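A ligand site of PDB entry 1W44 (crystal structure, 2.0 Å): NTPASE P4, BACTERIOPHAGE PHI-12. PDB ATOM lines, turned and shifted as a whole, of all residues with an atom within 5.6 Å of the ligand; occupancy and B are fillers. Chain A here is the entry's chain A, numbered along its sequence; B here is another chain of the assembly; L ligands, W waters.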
ATOM      1  N   ASN A 133      12.618 -29.376   0.897  1.00  0.00           N
ATOM      2  CA  ASN A 133      12.742 -28.666  -0.356  1.00  0.00           C
ATOM      3  C   ASN A 133      11.600 -28.820  -1.327  1.00  0.00           C
ATOM      4  O   ASN A 133      11.366 -27.933  -2.147  1.00  0.00           O
ATOM      5  CB  ASN A 133      14.080 -29.028  -1.031  1.00  0.00           C
ATOM      6  CG  ASN A 133      15.288 -28.469  -0.265  1.00  0.00           C
ATOM      7  OD1 ASN A 133      15.270 -27.310   0.178  1.00  0.00           O
ATOM      8  ND2 ASN A 133      16.335 -29.276  -0.127  1.00  0.00           N
ATOM      9  N   SER A 134      10.857 -29.915  -1.248  1.00  0.00           N
ATOM     10  CA  SER A 134       9.756 -30.101  -2.178  1.00  0.00           C
ATOM     11  C   SER A 134       8.825 -28.873  -2.145  1.00  0.00           C
ATOM     12  O   SER A 134       8.288 -28.509  -1.110  1.00  0.00           O
ATOM     13  CB  SER A 134       9.010 -31.390  -1.831  1.00  0.00           C
ATOM     14  OG  SER A 134       9.847 -32.500  -2.131  1.00  0.00           O
ATOM     15  N   GLY A 135       8.677 -28.238  -3.309  1.00  0.00           N
ATOM     16  CA  GLY A 135       7.872 -27.024  -3.445  1.00  0.00           C
ATOM     17  C   GLY A 135       6.389 -27.295  -3.363  1.00  0.00           C
ATOM     18  O   GLY A 135       5.870 -28.183  -4.041  1.00  0.00           O
ATOM     19  N   LYS A 136       5.682 -26.497  -2.574  1.00  0.00           N
ATOM     20  CA  LYS A 136       4.234 -26.709  -2.410  1.00  0.00           C
ATOM     21  C   LYS A 136       3.380 -26.162  -3.537  1.00  0.00           C
ATOM     22  O   LYS A 136       2.453 -26.829  -3.990  1.00  0.00           O
ATOM     23  CB  LYS A 136       3.782 -26.132  -1.055  1.00  0.00           C
ATOM     24  CG  LYS A 136       4.550 -26.766   0.096  1.00  0.00           C
ATOM     25  CD  LYS A 136       4.295 -26.083   1.395  1.00  0.00           C
ATOM     26  CE  LYS A 136       5.232 -26.592   2.462  1.00  0.00           C
ATOM     27  NZ  LYS A 136       6.617 -26.082   2.274  1.00  0.00           N
ATOM     28  N   THR A 137       3.680 -24.937  -3.973  1.00  0.00           N
ATOM     29  CA  THR A 137       2.912 -24.329  -5.059  1.00  0.00           C
ATOM     30  C   THR A 137       2.854 -25.205  -6.305  1.00  0.00           C
ATOM     31  O   THR A 137       1.763 -25.436  -6.839  1.00  0.00           O
ATOM     32  CB  THR A 137       3.461 -22.921  -5.344  1.00  0.00           C
ATOM     33  OG1 THR A 137       3.206 -22.121  -4.191  1.00  0.00           O
ATOM     34  CG2 THR A 137       2.798 -22.262  -6.579  1.00  0.00           C
ATOM     35  N   PRO A 138       4.012 -25.740  -6.760  1.00  0.00           N
ATOM     36  CA  PRO A 138       3.935 -26.590  -7.962  1.00  0.00           C
ATOM     37  C   PRO A 138       3.064 -27.808  -7.709  1.00  0.00           C
ATOM     38  O   PRO A 138       2.374 -28.287  -8.608  1.00  0.00           O
ATOM     39  CB  PRO A 138       5.399 -26.984  -8.209  1.00  0.00           C
ATOM     40  CG  PRO A 138       6.157 -25.809  -7.660  1.00  0.00           C
ATOM     41  CD  PRO A 138       5.418 -25.501  -6.371  1.00  0.00           C
ATOM     42  N   GLU A 160       0.316 -13.146  -1.796  1.00  0.00           N
ATOM     43  CA  GLU A 160       1.697 -13.399  -2.198  1.00  0.00           C
ATOM     44  C   GLU A 160       2.161 -12.066  -2.798  1.00  0.00           C
ATOM     45  O   GLU A 160       1.372 -11.358  -3.438  1.00  0.00           O
ATOM     46  CB  GLU A 160       1.781 -14.511  -3.257  1.00  0.00           C
ATOM     47  CG  GLU A 160       1.582 -15.939  -2.718  1.00  0.00           C
ATOM     48  CD  GLU A 160       2.638 -16.346  -1.711  1.00  0.00           C
ATOM     49  OE1 GLU A 160       2.460 -16.105  -0.502  1.00  0.00           O
ATOM     50  OE2 GLU A 160       3.665 -16.909  -2.137  1.00  0.00           O
ATOM     51  N   ASP A 189      -3.946 -20.462  -3.614  1.00  0.00           N
ATOM     52  CA  ASP A 189      -2.530 -20.259  -3.547  1.00  0.00           C
ATOM     53  C   ASP A 189      -2.342 -19.185  -2.554  1.00  0.00           C
ATOM     54  O   ASP A 189      -2.606 -17.995  -2.808  1.00  0.00           O
ATOM     55  CB  ASP A 189      -1.879 -19.863  -4.869  1.00  0.00           C
ATOM     56  CG  ASP A 189      -0.406 -20.221  -4.914  1.00  0.00           C
ATOM     57  OD1 ASP A 189       0.259 -20.140  -3.852  1.00  0.00           O
ATOM     58  OD2 ASP A 189       0.103 -20.576  -6.006  1.00  0.00           O
ATOM     59  N   LYS A 192      -1.393 -19.061   3.629  1.00  0.00           N
ATOM     60  CA  LYS A 192      -0.401 -18.457   4.512  1.00  0.00           C
ATOM     61  C   LYS A 192      -0.770 -17.146   5.198  1.00  0.00           C
ATOM     62  O   LYS A 192      -0.377 -16.902   6.343  1.00  0.00           O
ATOM     63  CB  LYS A 192       0.920 -18.242   3.750  1.00  0.00           C
ATOM     64  CG  LYS A 192       1.830 -19.467   3.754  1.00  0.00           C
ATOM     65  CD  LYS A 192       3.166 -19.178   3.047  1.00  0.00           C
ATOM     66  CE  LYS A 192       3.048 -19.327   1.535  1.00  0.00           C
ATOM     67  NZ  LYS A 192       2.630 -20.725   1.189  1.00  0.00           N
ATOM     68  N   ASN A 234       2.758 -23.071   4.402  1.00  0.00           N
ATOM     69  CA  ASN A 234       4.159 -23.241   4.805  1.00  0.00           C
ATOM     70  C   ASN A 234       4.329 -23.193   6.317  1.00  0.00           C
ATOM     71  O   ASN A 234       4.051 -22.172   6.950  1.00  0.00           O
ATOM     72  CB  ASN A 234       5.040 -22.179   4.140  1.00  0.00           C
ATOM     73  CG  ASN A 234       5.384 -22.524   2.698  1.00  0.00           C
ATOM     74  OD1 ASN A 234       4.492 -22.668   1.865  1.00  0.00           O
ATOM     75  ND2 ASN A 234       6.677 -22.665   2.410  1.00  0.00           N
ATOM     76  N   TYR A 288       9.715 -32.429 -12.224  1.00  0.00           N
ATOM     77  CA  TYR A 288       9.539 -31.165 -12.920  1.00  0.00           C
ATOM     78  C   TYR A 288       9.818 -31.224 -14.417  1.00  0.00           C
ATOM     79  O   TYR A 288      10.741 -31.908 -14.839  1.00  0.00           O
ATOM     80  CB  TYR A 288      10.465 -30.104 -12.315  1.00  0.00           C
ATOM     81  CG  TYR A 288      10.061 -29.612 -10.952  1.00  0.00           C
ATOM     82  CD1 TYR A 288       9.085 -28.642 -10.807  1.00  0.00           C
ATOM     83  CD2 TYR A 288      10.676 -30.108  -9.795  1.00  0.00           C
ATOM     84  CE1 TYR A 288       8.726 -28.167  -9.556  1.00  0.00           C
ATOM     85  CE2 TYR A 288      10.317 -29.645  -8.533  1.00  0.00           C
ATOM     86  CZ  TYR A 288       9.338 -28.660  -8.431  1.00  0.00           C
ATOM     87  OH  TYR A 288       8.975 -28.168  -7.213  1.00  0.00           O
ATOM     88  N   GLY A 289       9.018 -30.491 -15.185  1.00  0.00           N
ATOM     89  CA  GLY A 289       9.218 -30.379 -16.624  1.00  0.00           C
ATOM     90  C   GLY A 289       9.738 -28.952 -16.845  1.00  0.00           C
ATOM     91  O   GLY A 289      10.485 -28.437 -16.010  1.00  0.00           O
ATOM     92  N   SER A 292       8.997 -25.092 -14.361  1.00  0.00           N
ATOM     93  CA  SER A 292       8.508 -25.581 -13.090  1.00  0.00           C
ATOM     94  C   SER A 292       7.136 -26.268 -13.105  1.00  0.00           C
ATOM     95  O   SER A 292       6.485 -26.343 -12.065  1.00  0.00           O
ATOM     96  CB  SER A 292       8.460 -24.420 -12.070  1.00  0.00           C
ATOM     97  OG  SER A 292       9.739 -23.857 -11.875  1.00  0.00           O
ATOM     98  N   ARG B 272      12.654 -13.966  -5.960  1.00  0.00           N
ATOM     99  CA  ARG B 272      11.571 -14.869  -6.357  1.00  0.00           C
ATOM    100  C   ARG B 272      11.284 -14.420  -7.804  1.00  0.00           C
ATOM    101  O   ARG B 272      10.950 -13.253  -8.058  1.00  0.00           O
ATOM    102  CB  ARG B 272      10.302 -14.676  -5.506  1.00  0.00           C
ATOM    103  CG  ARG B 272      10.403 -15.173  -4.070  1.00  0.00           C
ATOM    104  CD  ARG B 272       9.098 -15.001  -3.285  1.00  0.00           C
ATOM    105  NE  ARG B 272       7.988 -15.778  -3.844  1.00  0.00           N
ATOM    106  CZ  ARG B 272       6.798 -15.885  -3.263  1.00  0.00           C
ATOM    107  NH1 ARG B 272       6.581 -15.262  -2.124  1.00  0.00           N
ATOM    108  NH2 ARG B 272       5.829 -16.605  -3.801  1.00  0.00           N
ATOM    109  N   GLY B 274       8.910 -15.655  -9.816  1.00  0.00           N
ATOM    110  CA  GLY B 274       7.514 -15.776 -10.195  1.00  0.00           C
ATOM    111  C   GLY B 274       6.765 -16.865  -9.431  1.00  0.00           C
ATOM    112  O   GLY B 274       7.328 -17.621  -8.655  1.00  0.00           O
ATOM    113  N   GLU B 275       5.470 -16.965  -9.701  1.00  0.00           N
ATOM    114  CA  GLU B 275       4.603 -17.950  -9.063  1.00  0.00           C
ATOM    115  C   GLU B 275       5.088 -19.372  -9.355  1.00  0.00           C
ATOM    116  O   GLU B 275       5.162 -19.787 -10.524  1.00  0.00           O
ATOM    117  CB  GLU B 275       3.178 -17.770  -9.584  1.00  0.00           C
ATOM    118  CG  GLU B 275       2.142 -18.713  -9.055  1.00  0.00           C
ATOM    119  CD  GLU B 275       0.769 -18.346  -9.627  1.00  0.00           C
ATOM    120  OE1 GLU B 275       0.414 -18.843 -10.716  1.00  0.00           O
ATOM    121  OE2 GLU B 275       0.072 -17.537  -8.980  1.00  0.00           O
ATOM    122  N   GLY B 276       5.399 -20.100  -8.293  1.00  0.00           N
ATOM    123  CA  GLY B 276       5.842 -21.472  -8.435  1.00  0.00           C
ATOM    124  C   GLY B 276       7.221 -21.667  -9.038  1.00  0.00           C
ATOM    125  O   GLY B 276       7.630 -22.812  -9.232  1.00  0.00           O
ATOM    126  N   LEU B 277       7.932 -20.579  -9.298  1.00  0.00           N
ATOM    127  CA  LEU B 277       9.248 -20.690  -9.912  1.00  0.00           C
ATOM    128  C   LEU B 277      10.364 -20.681  -8.868  1.00  0.00           C
ATOM    129  O   LEU B 277      10.131 -20.435  -7.680  1.00  0.00           O
ATOM    130  CB  LEU B 277       9.460 -19.579 -10.947  1.00  0.00           C
ATOM    131  CG  LEU B 277       8.308 -19.424 -11.965  1.00  0.00           C
ATOM    132  CD1 LEU B 277       8.626 -18.295 -12.919  1.00  0.00           C
ATOM    133  CD2 LEU B 277       8.068 -20.715 -12.760  1.00  0.00           C
ATOM    134  N   GLN B 278      11.584 -20.975  -9.307  1.00  0.00           N
ATOM    135  CA  GLN B 278      12.734 -21.026  -8.413  1.00  0.00           C
ATOM    136  C   GLN B 278      13.257 -19.670  -8.001  1.00  0.00           C
ATOM    137  O   GLN B 278      13.165 -18.691  -8.761  1.00  0.00           O
ATOM    138  CB  GLN B 278      13.872 -21.800  -9.071  1.00  0.00           C
ATOM    139  CG  GLN B 278      13.813 -23.309  -8.844  1.00  0.00           C
ATOM    140  CD  GLN B 278      14.599 -24.108  -9.874  1.00  0.00           C
ATOM    141  OE1 GLN B 278      15.215 -25.113  -9.552  1.00  0.00           O
ATOM    142  NE2 GLN B 278      14.560 -23.651 -11.131  1.00  0.00           N
ATOM    143  N   ARG B 279      13.779 -19.600  -6.780  1.00  0.00           N
ATOM    144  CA  ARG B 279      14.403 -18.385  -6.282  1.00  0.00           C
ATOM    145  C   ARG B 279      15.835 -18.398  -6.813  1.00  0.00           C
ATOM    146  O   ARG B 279      16.481 -19.451  -6.828  1.00  0.00           O
ATOM    147  CB  ARG B 279      14.450 -18.359  -4.759  1.00  0.00           C
ATOM    148  CG  ARG B 279      13.221 -17.829  -4.062  1.00  0.00           C
ATOM    149  CD  ARG B 279      13.561 -17.495  -2.619  1.00  0.00           C
ATOM    150  NE  ARG B 279      12.345 -17.428  -1.796  1.00  0.00           N
ATOM    151  CZ  ARG B 279      11.862 -16.313  -1.275  1.00  0.00           C
ATOM    152  NH1 ARG B 279      12.487 -15.164  -1.476  1.00  0.00           N
ATOM    153  NH2 ARG B 279      10.740 -16.350  -0.565  1.00  0.00           N
ATOM    154  N   SER B 308      18.478 -21.524  -6.019  1.00  0.00           N
ATOM    155  CA  SER B 308      18.665 -22.020  -4.658  1.00  0.00           C
ATOM    156  C   SER B 308      17.404 -22.744  -4.155  1.00  0.00           C
ATOM    157  O   SER B 308      16.288 -22.472  -4.616  1.00  0.00           O
ATOM    158  CB  SER B 308      19.038 -20.870  -3.709  1.00  0.00           C
ATOM    159  OG  SER B 308      17.947 -19.992  -3.494  1.00  0.00           O
ATOM    160  N   GLY B 309      17.591 -23.687  -3.226  1.00  0.00           N
ATOM    161  CA  GLY B 309      16.469 -24.454  -2.693  1.00  0.00           C
ATOM    162  C   GLY B 309      15.920 -23.890  -1.396  1.00  0.00           C
ATOM    163  O   GLY B 309      16.555 -23.049  -0.752  1.00  0.00           O
ATOM    164  N   LYS B 310      14.732 -24.353  -1.001  1.00  0.00           N
ATOM    165  CA  LYS B 310      14.088 -23.890   0.227  1.00  0.00           C
ATOM    166  C   LYS B 310      15.007 -23.990   1.451  1.00  0.00           C
ATOM    167  O   LYS B 310      14.986 -23.106   2.312  1.00  0.00           O
ATOM    168  CB  LYS B 310      12.799 -24.673   0.485  1.00  0.00           C
ATOM    169  CG  LYS B 310      11.577 -23.793   0.623  1.00  0.00           C
ATOM    170  CD  LYS B 310      11.385 -22.936  -0.615  1.00  0.00           C
ATOM    171  CE  LYS B 310      10.133 -22.072  -0.502  1.00  0.00           C
ATOM    172  NZ  LYS B 310      10.017 -21.136  -1.662  1.00  0.00           N
HETATM  173  P1  LIG L   1       6.887 -23.142  -1.830  1.00  0.00           P
HETATM  174  O1  LIG L   1       6.521 -22.374  -0.592  1.00  0.00           O
HETATM  175  O2  LIG L   1       8.016 -24.239  -1.573  1.00  0.00           O
HETATM  176  O3  LIG L   1       5.702 -23.813  -2.385  1.00  0.00           O
HETATM  177  P2  LIG L   1       6.901 -21.235  -4.015  1.00  0.00           P
HETATM  178  O4  LIG L   1       7.737 -20.092  -4.205  1.00  0.00           O
HETATM  179  O5  LIG L   1       5.527 -20.808  -3.723  1.00  0.00           O
HETATM  180  O6  LIG L   1       7.492 -22.124  -2.871  1.00  0.00           O
HETATM  181  O7  LIG L   1       6.891 -22.259  -5.236  1.00  0.00           O
HETATM  182  C1  LIG L   1       8.119 -22.707  -5.707  1.00  0.00           C
HETATM  183  C2  LIG L   1       8.669 -23.996  -5.131  1.00  0.00           C
HETATM  184  O8  LIG L   1       8.931 -24.979  -6.160  1.00  0.00           O
HETATM  185  C3  LIG L   1       9.944 -23.655  -4.502  1.00  0.00           C
HETATM  186  O9  LIG L   1      10.159 -24.367  -3.276  1.00  0.00           O
HETATM  187  C4  LIG L   1      10.963 -23.954  -5.573  1.00  0.00           C
HETATM  188  O10 LIG L   1      12.272 -24.023  -5.026  1.00  0.00           O
HETATM  189  C5  LIG L   1      10.380 -25.232  -6.201  1.00  0.00           C
HETATM  190  N1  LIG L   1      10.764 -25.444  -7.660  1.00  0.00           N
HETATM  191  C6  LIG L   1      10.204 -24.806  -8.720  1.00  0.00           C
HETATM  192  N2  LIG L   1      10.757 -25.241  -9.866  1.00  0.00           N
HETATM  193  C7  LIG L   1      11.637 -26.129  -9.578  1.00  0.00           C
HETATM  194  C8  LIG L   1      12.499 -26.908 -10.319  1.00  0.00           C
HETATM  195  N3  LIG L   1      12.505 -26.819 -11.628  1.00  0.00           N
HETATM  196  N4  LIG L   1      13.340 -27.778  -9.702  1.00  0.00           N
HETATM  197  C9  LIG L   1      13.371 -27.921  -8.348  1.00  0.00           C
HETATM  198  N5  LIG L   1      12.532 -27.160  -7.600  1.00  0.00           N
HETATM  199  C10 LIG L   1      11.663 -26.271  -8.153  1.00  0.00           C
HETATM  200  O   HOH W   1       8.553 -18.408  -2.246  1.00  0.00           O
HETATM  201  O   HOH W   2       4.599 -19.648  -1.377  1.00  0.00           O
HETATM  202  O   HOH W   3      12.881 -25.575  -2.688  1.00  0.00           O
HETATM  203  O   HOH W   4      11.580 -26.341 -14.308  1.00  0.00           O
HETATM  204  O   HOH W   5       4.922 -18.945  -5.736  1.00  0.00           O
HETATM  205  O   HOH W   6      10.528 -29.008  -5.427  1.00  0.00           O
HETATM  206  O   HOH W   7      14.405 -29.056 -13.094  1.00  0.00           O
HETATM  207  O   HOH W   8       3.303 -22.342  -0.828  1.00  0.00           O
HETATM  208  O   HOH W   9      13.762 -21.870  -4.874  1.00  0.00           O
HETATM  209  O   HOH W  10       7.952 -17.878  -5.863  1.00  0.00           O
HETATM  210  O   HOH W  11      10.581 -20.278  -4.475  1.00  0.00           O
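Asn 133 touches the ligand.
Gly 135 touches the ligand.
CG of Pro 138 touches O8 of the ligand, at 3.3 Å.
O of Gly 276 of chain B touches C6 of the ligand (3.3 Å).
Leu 277 of chain B touches the ligand.
Hydrophobic or aromatic side chains that line the ligand: Pro 138 and Tyr 288.
Of the 23 residues printed, 13 come within 4 Å of the ligand.
Along chain A the residues within 4 Å of the ligand span positions 133 to 292.
The nearest printed residue that does not touch the ligand is Ser 134 (4.3 Å).
Water W9 lies within hydrogen-bond range of O of Ser 308 of chain B (2.6 Å), O10 of the ligand (2.6 Å) and N of Arg 279 of chain B (3.0 Å).
Water W5 lies within hydrogen-bond range of O5 of the ligand, N of Gly 276 of chain B and NH2 of Arg 272 of chain B.
Water W11 lies within hydrogen-bond range of O4 of the ligand, NZ of Lys 310 of chain B and O of Leu 277 of chain B.
Water W4 lies within hydrogen-bond range of N of Ser 292 (2.9 Å), N3 of the ligand (2.9 Å) and O of Gly 289 (2.9 Å).
Water W8 lies within hydrogen-bond range of the side-chain amino group of Lys 192 (2.7 Å), the side-chain amide oxygen of Asn 234 (3.0 Å), an oxygen (O3) of the ligand (3.2 Å) and the side-chain hydroxyl of Thr 137 (3.4 Å).
Water W6 lies within hydrogen-bond range of OH of Tyr 288 (2.5 Å), N of Gly 135 (2.9 Å) and N5 of the ligand (3.5 Å).
An oxygen (O3) of the ligand lies within hydrogen-bond range of the backbone NH (N) of Lys 136 (2.7 Å).
A nitrogen (N4) of the ligand lies close to the side-chain amide oxygen (OE1) of Gln 278 of chain B, at 3.3 Å.
The side-chain hydroxyl (OG) of Ser 292 sits at hydrogen-bond distance from a nitrogen (N2) of the ligand (2.6 Å).
The side-chain hydroxyl (OG1) of Thr 137 is in hydrogen-bond range of an oxygen (O5) of the ligand (2.7 Å).
An oxygen (O4) of the ligand is in salt-bridge range of the guanidinium group of Arg 272 of chain B, 3.995 Å away.
The side-chain amide nitrogen (ND2) of Asn 234 sits at hydrogen-bond distance from an oxygen (O1) of the ligand.
An oxygen (O8) of the ligand sits at hydrogen-bond distance from the side-chain hydroxyl (OH) of Tyr 288 (3.4 Å).
NZ of Lys 310 of chain B is in salt-bridge range of O4 of the ligand, at 3.6 Å.
An oxygen (O3) of the ligand sits at hydrogen-bond distance from the backbone NH (N) of Thr 137.
The side-chain carboxylate (OE2) of Glu 160 is in salt-bridge range of the guanidinium group (NH2) of Arg 272 of chain B, at 2.7 Å.
The side-chain amino group (NZ) of Lys 192 is in hydrogen-bond range of the side-chain amide oxygen (OD1) of Asn 234 (2.8 Å).
The side-chain amino group (NZ) of Lys 136 lies close to the side-chain amide nitrogen (ND2) of Asn 234, 3.4 Å away.
N of Lys 310 of chain B lies within hydrogen-bond range of OD1 of Asn 133, 3.2 Å away.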
